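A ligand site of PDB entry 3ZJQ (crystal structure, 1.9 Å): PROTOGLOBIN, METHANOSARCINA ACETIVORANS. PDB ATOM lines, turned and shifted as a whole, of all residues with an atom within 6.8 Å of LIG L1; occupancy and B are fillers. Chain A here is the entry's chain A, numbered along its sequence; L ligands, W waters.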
ATOM      1  N   LEU A  57       7.546  26.988   0.859  1.00  0.00           N
ATOM      2  CA  LEU A  57       7.712  27.653  -0.430  1.00  0.00           C
ATOM      3  C   LEU A  57       8.868  27.063  -1.238  1.00  0.00           C
ATOM      4  O   LEU A  57       8.746  26.878  -2.450  1.00  0.00           O
ATOM      5  CB  LEU A  57       7.933  29.153  -0.219  1.00  0.00           C
ATOM      6  CG  LEU A  57       6.790  30.177  -0.306  1.00  0.00           C
ATOM      7  CD1 LEU A  57       5.391  29.594  -0.178  1.00  0.00           C
ATOM      8  CD2 LEU A  57       7.028  31.269   0.735  1.00  0.00           C
ATOM      9  N   THR A  59      10.068  24.041  -1.126  1.00  0.00           N
ATOM     10  CA  THR A  59       9.659  22.716  -1.606  1.00  0.00           C
ATOM     11  C   THR A  59       8.771  22.844  -2.845  1.00  0.00           C
ATOM     12  O   THR A  59       8.987  22.149  -3.835  1.00  0.00           O
ATOM     13  CB  THR A  59       8.911  21.926  -0.511  1.00  0.00           C
ATOM     14  OG1 THR A  59       9.678  21.916   0.690  1.00  0.00           O
ATOM     15  CG2 THR A  59       8.673  20.476  -0.945  1.00  0.00           C
ATOM     16  N   TRP A  60       7.780  23.734  -2.788  1.00  0.00           N
ATOM     17  CA  TRP A  60       6.851  23.917  -3.886  1.00  0.00           C
ATOM     18  C   TRP A  60       7.536  24.523  -5.101  1.00  0.00           C
ATOM     19  O   TRP A  60       7.317  24.082  -6.236  1.00  0.00           O
ATOM     20  CB  TRP A  60       5.637  24.761  -3.457  1.00  0.00           C
ATOM     21  CG  TRP A  60       4.688  24.040  -2.510  1.00  0.00           C
ATOM     22  CD1 TRP A  60       4.581  22.695  -2.329  1.00  0.00           C
ATOM     23  CD2 TRP A  60       3.704  24.639  -1.670  1.00  0.00           C
ATOM     24  NE1 TRP A  60       3.610  22.413  -1.399  1.00  0.00           N
ATOM     25  CE2 TRP A  60       3.048  23.589  -0.980  1.00  0.00           C
ATOM     26  CE3 TRP A  60       3.321  25.962  -1.408  1.00  0.00           C
ATOM     27  CZ2 TRP A  60       2.028  23.828  -0.062  1.00  0.00           C
ATOM     28  CZ3 TRP A  60       2.294  26.189  -0.495  1.00  0.00           C
ATOM     29  CH2 TRP A  60       1.662  25.125   0.172  1.00  0.00           C
ATOM     30  N   TYR A  61       8.378  25.519  -4.862  1.00  0.00           N
ATOM     31  CA  TYR A  61       9.151  26.159  -5.915  1.00  0.00           C
ATOM     32  C   TYR A  61      10.201  25.240  -6.532  1.00  0.00           C
ATOM     33  O   TYR A  61      10.510  25.343  -7.729  1.00  0.00           O
ATOM     34  CB  TYR A  61       9.776  27.466  -5.419  1.00  0.00           C
ATOM     35  CG  TYR A  61       8.940  28.695  -5.722  1.00  0.00           C
ATOM     36  CD1 TYR A  61       7.667  28.847  -5.166  1.00  0.00           C
ATOM     37  CD2 TYR A  61       9.416  29.698  -6.559  1.00  0.00           C
ATOM     38  CE1 TYR A  61       6.885  29.970  -5.451  1.00  0.00           C
ATOM     39  CE2 TYR A  61       8.648  30.819  -6.839  1.00  0.00           C
ATOM     40  CZ  TYR A  61       7.392  30.956  -6.291  1.00  0.00           C
ATOM     41  OH  TYR A  61       6.644  32.069  -6.601  1.00  0.00           O
ATOM     42  N   GLY A  62      10.739  24.330  -5.710  1.00  0.00           N
ATOM     43  CA  GLY A  62      11.718  23.350  -6.170  1.00  0.00           C
ATOM     44  C   GLY A  62      11.087  22.312  -7.077  1.00  0.00           C
ATOM     45  O   GLY A  62      11.694  21.869  -8.055  1.00  0.00           O
ATOM     46  N   PHE A  63       9.852  21.923  -6.758  1.00  0.00           N
ATOM     47  CA  PHE A  63       9.073  21.029  -7.616  1.00  0.00           C
ATOM     48  C   PHE A  63       8.841  21.663  -8.987  1.00  0.00           C
ATOM     49  O   PHE A  63       9.137  21.045 -10.008  1.00  0.00           O
ATOM     50  CB  PHE A  63       7.751  20.652  -6.946  1.00  0.00           C
ATOM     51  CG  PHE A  63       6.791  19.925  -7.856  1.00  0.00           C
ATOM     52  CD1 PHE A  63       7.112  18.669  -8.358  1.00  0.00           C
ATOM     53  CD2 PHE A  63       5.563  20.496  -8.184  1.00  0.00           C
ATOM     54  CE1 PHE A  63       6.221  17.990  -9.206  1.00  0.00           C
ATOM     55  CE2 PHE A  63       4.665  19.815  -9.017  1.00  0.00           C
ATOM     56  CZ  PHE A  63       4.992  18.569  -9.528  1.00  0.00           C
ATOM     57  N   VAL A  64       8.307  22.885  -9.006  1.00  0.00           N
ATOM     58  CA  VAL A  64       8.020  23.597 -10.251  1.00  0.00           C
ATOM     59  C   VAL A  64       9.304  23.849 -11.055  1.00  0.00           C
ATOM     60  O   VAL A  64       9.320  23.676 -12.281  1.00  0.00           O
ATOM     61  CB  VAL A  64       7.244  24.928 -10.007  1.00  0.00           C
ATOM     62  CG1 VAL A  64       7.350  25.882 -11.196  1.00  0.00           C
ATOM     63  CG2 VAL A  64       5.777  24.636  -9.707  1.00  0.00           C
ATOM     64  N   GLY A  65      10.364  24.227 -10.349  1.00  0.00           N
ATOM     65  CA  GLY A  65      11.658  24.523 -10.966  1.00  0.00           C
ATOM     66  C   GLY A  65      12.339  23.322 -11.615  1.00  0.00           C
ATOM     67  O   GLY A  65      13.131  23.484 -12.543  1.00  0.00           O
ATOM     68  N   PHE A  74       6.284  30.744 -15.668  1.00  0.00           N
ATOM     69  CA  PHE A  74       6.974  31.928 -15.147  1.00  0.00           C
ATOM     70  C   PHE A  74       8.029  32.462 -16.123  1.00  0.00           C
ATOM     71  O   PHE A  74       8.810  33.335 -15.760  1.00  0.00           O
ATOM     72  CB  PHE A  74       7.661  31.605 -13.812  1.00  0.00           C
ATOM     73  CG  PHE A  74       6.717  31.364 -12.669  1.00  0.00           C
ATOM     74  CD1 PHE A  74       6.252  32.429 -11.898  1.00  0.00           C
ATOM     75  CD2 PHE A  74       6.340  30.064 -12.333  1.00  0.00           C
ATOM     76  CE1 PHE A  74       5.387  32.205 -10.827  1.00  0.00           C
ATOM     77  CE2 PHE A  74       5.478  29.834 -11.253  1.00  0.00           C
ATOM     78  CZ  PHE A  74       4.996  30.906 -10.496  1.00  0.00           C
ATOM     79  N   LEU A  86       8.728  35.358 -10.512  1.00  0.00           N
ATOM     80  CA  LEU A  86       8.771  34.288  -9.514  1.00  0.00           C
ATOM     81  C   LEU A  86       8.758  34.829  -8.087  1.00  0.00           C
ATOM     82  O   LEU A  86       8.003  34.337  -7.249  1.00  0.00           O
ATOM     83  CB  LEU A  86       9.984  33.375  -9.736  1.00  0.00           C
ATOM     84  CG  LEU A  86       9.880  32.276 -10.802  1.00  0.00           C
ATOM     85  CD1 LEU A  86      11.259  31.885 -11.342  1.00  0.00           C
ATOM     86  CD2 LEU A  86       9.162  31.056 -10.250  1.00  0.00           C
ATOM     87  N   VAL A  89       5.328  36.778  -7.056  1.00  0.00           N
ATOM     88  CA  VAL A  89       4.271  35.788  -6.824  1.00  0.00           C
ATOM     89  C   VAL A  89       4.498  35.043  -5.514  1.00  0.00           C
ATOM     90  O   VAL A  89       3.532  34.779  -4.776  1.00  0.00           O
ATOM     91  CB  VAL A  89       4.159  34.785  -8.021  1.00  0.00           C
ATOM     92  CG1 VAL A  89       3.200  33.644  -7.721  1.00  0.00           C
ATOM     93  CG2 VAL A  89       3.741  35.516  -9.301  1.00  0.00           C
ATOM     94  N   ARG A  90       5.757  34.723  -5.216  1.00  0.00           N
ATOM     95  CA  ARG A  90       6.132  34.005  -3.997  1.00  0.00           C
ATOM     96  C   ARG A  90       5.588  34.678  -2.747  1.00  0.00           C
ATOM     97  O   ARG A  90       5.117  34.010  -1.827  1.00  0.00           O
ATOM     98  CB  ARG A  90       7.665  33.851  -3.895  1.00  0.00           C
ATOM     99  CG  ARG A  90       8.129  32.835  -2.865  1.00  0.00           C
ATOM    100  CD  ARG A  90       9.650  32.716  -2.840  1.00  0.00           C
ATOM    101  NE  ARG A  90      10.120  31.960  -1.686  1.00  0.00           N
ATOM    102  CZ  ARG A  90      10.754  30.796  -1.749  1.00  0.00           C
ATOM    103  NH1 ARG A  90      11.006  30.222  -2.929  1.00  0.00           N
ATOM    104  NH2 ARG A  90      11.134  30.190  -0.628  1.00  0.00           N
ATOM    105  N   PHE A  93       1.831  34.126  -2.684  1.00  0.00           N
ATOM    106  CA  PHE A  93       1.658  32.690  -2.435  1.00  0.00           C
ATOM    107  C   PHE A  93       1.864  32.379  -0.946  1.00  0.00           C
ATOM    108  O   PHE A  93       1.114  31.599  -0.351  1.00  0.00           O
ATOM    109  CB  PHE A  93       2.676  31.916  -3.295  1.00  0.00           C
ATOM    110  CG  PHE A  93       2.384  30.434  -3.427  1.00  0.00           C
ATOM    111  CD1 PHE A  93       1.094  29.933  -3.342  1.00  0.00           C
ATOM    112  CD2 PHE A  93       3.424  29.559  -3.688  1.00  0.00           C
ATOM    113  CE1 PHE A  93       0.841  28.573  -3.492  1.00  0.00           C
ATOM    114  CE2 PHE A  93       3.183  28.195  -3.846  1.00  0.00           C
ATOM    115  CZ  PHE A  93       1.882  27.698  -3.753  1.00  0.00           C
ATOM    116  N   HIS A 120      -4.555  33.161 -12.767  1.00  0.00           N
ATOM    117  CA  HIS A 120      -3.965  31.986 -13.414  1.00  0.00           C
ATOM    118  C   HIS A 120      -4.424  31.921 -14.864  1.00  0.00           C
ATOM    119  O   HIS A 120      -3.686  31.465 -15.736  1.00  0.00           O
ATOM    120  CB  HIS A 120      -4.328  30.674 -12.680  1.00  0.00           C
ATOM    121  CG  HIS A 120      -3.595  30.464 -11.399  1.00  0.00           C
ATOM    122  ND1 HIS A 120      -4.038  30.977 -10.196  1.00  0.00           N
ATOM    123  CD2 HIS A 120      -2.442  29.811 -11.127  1.00  0.00           C
ATOM    124  CE1 HIS A 120      -3.188  30.654  -9.246  1.00  0.00           C
ATOM    125  NE2 HIS A 120      -2.208  29.946  -9.771  1.00  0.00           N
ATOM    126  N   ILE A 137      -2.383  29.704 -17.961  1.00  0.00           N
ATOM    127  CA  ILE A 137      -2.001  28.436 -17.341  1.00  0.00           C
ATOM    128  C   ILE A 137      -3.101  27.415 -17.576  1.00  0.00           C
ATOM    129  O   ILE A 137      -4.206  27.538 -17.039  1.00  0.00           O
ATOM    130  CB  ILE A 137      -1.722  28.553 -15.823  1.00  0.00           C
ATOM    131  CG1 ILE A 137      -0.599  29.565 -15.554  1.00  0.00           C
ATOM    132  CG2 ILE A 137      -1.334  27.190 -15.232  1.00  0.00           C
ATOM    133  CD1 ILE A 137      -0.502  30.028 -14.109  1.00  0.00           C
ATOM    134  N   PHE A 145      -2.161  20.089  -9.543  1.00  0.00           N
ATOM    135  CA  PHE A 145      -1.420  20.624  -8.404  1.00  0.00           C
ATOM    136  C   PHE A 145      -2.109  20.441  -7.053  1.00  0.00           C
ATOM    137  O   PHE A 145      -1.481  20.649  -6.012  1.00  0.00           O
ATOM    138  CB  PHE A 145      -1.085  22.111  -8.627  1.00  0.00           C
ATOM    139  CG  PHE A 145       0.235  22.343  -9.316  1.00  0.00           C
ATOM    140  CD1 PHE A 145       0.705  21.475 -10.300  1.00  0.00           C
ATOM    141  CD2 PHE A 145       1.003  23.461  -8.992  1.00  0.00           C
ATOM    142  CE1 PHE A 145       1.930  21.710 -10.948  1.00  0.00           C
ATOM    143  CE2 PHE A 145       2.211  23.712  -9.632  1.00  0.00           C
ATOM    144  CZ  PHE A 145       2.676  22.835 -10.607  1.00  0.00           C
ATOM    145  N   PRO A 148       0.320  17.750  -5.319  1.00  0.00           N
ATOM    146  CA  PRO A 148       1.525  18.236  -4.644  1.00  0.00           C
ATOM    147  C   PRO A 148       1.266  19.298  -3.563  1.00  0.00           C
ATOM    148  O   PRO A 148       1.917  19.249  -2.513  1.00  0.00           O
ATOM    149  CB  PRO A 148       2.372  18.818  -5.793  1.00  0.00           C
ATOM    150  CG  PRO A 148       1.435  18.992  -6.945  1.00  0.00           C
ATOM    151  CD  PRO A 148       0.421  17.883  -6.780  1.00  0.00           C
ATOM    152  N   ILE A 149       0.334  20.225  -3.781  1.00  0.00           N
ATOM    153  CA  ILE A 149       0.030  21.258  -2.761  1.00  0.00           C
ATOM    154  C   ILE A 149      -0.522  20.648  -1.462  1.00  0.00           C
ATOM    155  O   ILE A 149      -0.224  21.139  -0.376  1.00  0.00           O
ATOM    156  CB  ILE A 149      -0.915  22.386  -3.314  1.00  0.00           C
ATOM    157  CG1 ILE A 149      -0.241  23.167  -4.455  1.00  0.00           C
ATOM    158  CG2 ILE A 149      -1.347  23.358  -2.186  1.00  0.00           C
ATOM    159  CD1 ILE A 149       1.065  23.867  -4.089  1.00  0.00           C
HETATM  160  N1  LIG L   1       1.445  28.949  -7.885  1.00  0.00           N
HETATM  161  C1  LIG L   1       1.922  27.715  -7.682  1.00  0.00           C
HETATM  162  C2  LIG L   1       3.240  27.560  -7.275  1.00  0.00           C
HETATM  163  C3  LIG L   1       4.052  28.673  -7.071  1.00  0.00           C
HETATM  164  C4  LIG L   1       3.529  29.946  -7.288  1.00  0.00           C
HETATM  165  C5  LIG L   1       2.215  30.047  -7.695  1.00  0.00           C
HETATM  166  C6  LIG L   1       3.803  26.191  -7.026  1.00  0.00           C
HETATM  167  O1  LIG L   1       3.042  25.238  -6.959  1.00  0.00           O
HETATM  168  N2  LIG L   1       5.117  26.057  -6.897  1.00  0.00           N
HETATM  169  C1  LG2 L   2      -0.268  32.752  -8.722  1.00  0.00           C
HETATM  170  C2  LG2 L   2      -1.510  29.214  -5.637  1.00  0.00           C
HETATM  171  C3  LG2 L   2      -1.651  26.255  -9.474  1.00  0.00           C
HETATM  172  C4  LG2 L   2       1.684  29.188 -11.408  1.00  0.00           C
HETATM  173  C5  LG2 L   2      -0.671  32.124  -7.558  1.00  0.00           C
HETATM  174  C6  LG2 L   2      -1.009  32.736  -6.277  1.00  0.00           C
HETATM  175  C7  LG2 L   2      -1.368  31.744  -5.443  1.00  0.00           C
HETATM  176  C8  LG2 L   2      -1.257  30.484  -6.139  1.00  0.00           C
HETATM  177  C9  LG2 L   2      -1.805  31.895  -3.973  1.00  0.00           C
HETATM  178  C10 LG2 L   2      -0.986  34.250  -5.960  1.00  0.00           C
HETATM  179  C11 LG2 L   2      -2.406  34.802  -5.968  1.00  0.00           C
HETATM  180  C12 LG2 L   2      -2.377  36.302  -5.758  1.00  0.00           C
HETATM  181  O1  LG2 L   2      -2.650  36.759  -4.621  1.00  0.00           O
HETATM  182  O2  LG2 L   2      -2.097  37.035  -6.741  1.00  0.00           O
HETATM  183  C13 LG2 L   2      -1.747  28.099  -6.415  1.00  0.00           C
HETATM  184  C14 LG2 L   2      -2.371  26.858  -5.995  1.00  0.00           C
HETATM  185  C15 LG2 L   2      -2.436  26.033  -7.054  1.00  0.00           C
HETATM  186  C16 LG2 L   2      -1.829  26.727  -8.179  1.00  0.00           C
HETATM  187  C17 LG2 L   2      -2.883  26.604  -4.564  1.00  0.00           C
HETATM  188  C18 LG2 L   2      -3.022  24.600  -7.137  1.00  0.00           C
HETATM  189  C19 LG2 L   2      -3.296  23.812  -6.088  1.00  0.00           C
HETATM  190  C20 LG2 L   2      -0.648  26.705 -10.305  1.00  0.00           C
HETATM  191  C21 LG2 L   2       0.013  26.001 -11.400  1.00  0.00           C
HETATM  192  C22 LG2 L   2       0.941  26.822 -11.919  1.00  0.00           C
HETATM  193  C23 LG2 L   2       0.910  28.068 -11.196  1.00  0.00           C
HETATM  194  C24 LG2 L   2      -0.296  24.574 -11.900  1.00  0.00           C
HETATM  195  C25 LG2 L   2       1.885  26.482 -13.092  1.00  0.00           C
HETATM  196  C26 LG2 L   2       3.197  26.552 -12.886  1.00  0.00           C
HETATM  197  C27 LG2 L   2       1.356  30.469 -11.032  1.00  0.00           C
HETATM  198  C28 LG2 L   2       1.714  31.706 -11.695  1.00  0.00           C
HETATM  199  C29 LG2 L   2       1.102  32.809 -10.845  1.00  0.00           C
HETATM  200  C30 LG2 L   2       0.418  32.146  -9.750  1.00  0.00           C
HETATM  201  C31 LG2 L   2       2.541  31.884 -12.993  1.00  0.00           C
HETATM  202  C32 LG2 L   2       1.135  34.325 -11.094  1.00  0.00           C
HETATM  203  C33 LG2 L   2      -0.098  34.593 -11.951  1.00  0.00           C
HETATM  204  C34 LG2 L   2      -0.206  36.054 -12.294  1.00  0.00           C
HETATM  205  O3  LG2 L   2       0.450  36.500 -13.270  1.00  0.00           O
HETATM  206  O4  LG2 L   2      -0.965  36.761 -11.583  1.00  0.00           O
HETATM  207  N1  LG2 L   2      -0.828  30.766  -7.425  1.00  0.00           N
HETATM  208  N2  LG2 L   2      -1.429  27.980  -7.743  1.00  0.00           N
HETATM  209  N3  LG2 L   2      -0.065  27.954 -10.228  1.00  0.00           N
HETATM  210  N4  LG2 L   2       0.596  30.777  -9.917  1.00  0.00           N
HETATM  211 FE1  LG2 L   2      -0.440  29.382  -8.827  1.00  0.00          FE
HETATM  212  O   HOH W   1       7.159  28.211  -8.643  1.00  0.00           O
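Tyr 61 touches LIG L1 (CE1 to C3, 3.5 Å).
Val 64 touches LIG L1 (CG2 to N2, 3.2 Å).
Phe 74 touches LIG L1.
CG1 of Val 89 touches C5 of LIG L1, at 3.7 Å.
Phe 93 touches LIG L1.
CE2 of Phe 145 touches O1 of LIG L1, 3.2 Å away.
Ile 149 touches LIG L1 (CD1 to O1, 3.7 Å).
Hydrophobic or aromatic side chains that line LIG L1: Trp 60, Tyr 61, Val 64, Phe 74, Val 89, Phe 93, Phe 145 and Ile 149.
Of the 18 residues printed, 8 come within 4 Å of LIG L1.
The nearest printed residue that does not touch LIG L1 is His 120 (4.2 Å).
A nitrogen (N1) of LIG L1 binds an iron atom (FE1) of LG2 L2 (2.2 Å).
The side-chain hydroxyl (OH) of Tyr 61 is in hydrogen-bond range of the backbone NH (N) of Arg 90, 3.1 Å away.
O of Leu 86 sits at hydrogen-bond distance from OH of Tyr 61 (2.7 Å).
A ring nitrogen (NE2) of His 120 binds an iron atom (FE1) of LG2 L2 (2.1 Å).
A nitrogen (N2) of LIG L1 sits at hydrogen-bond distance from the backbone carbonyl oxygen of Trp 60, at 3.0 Å.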
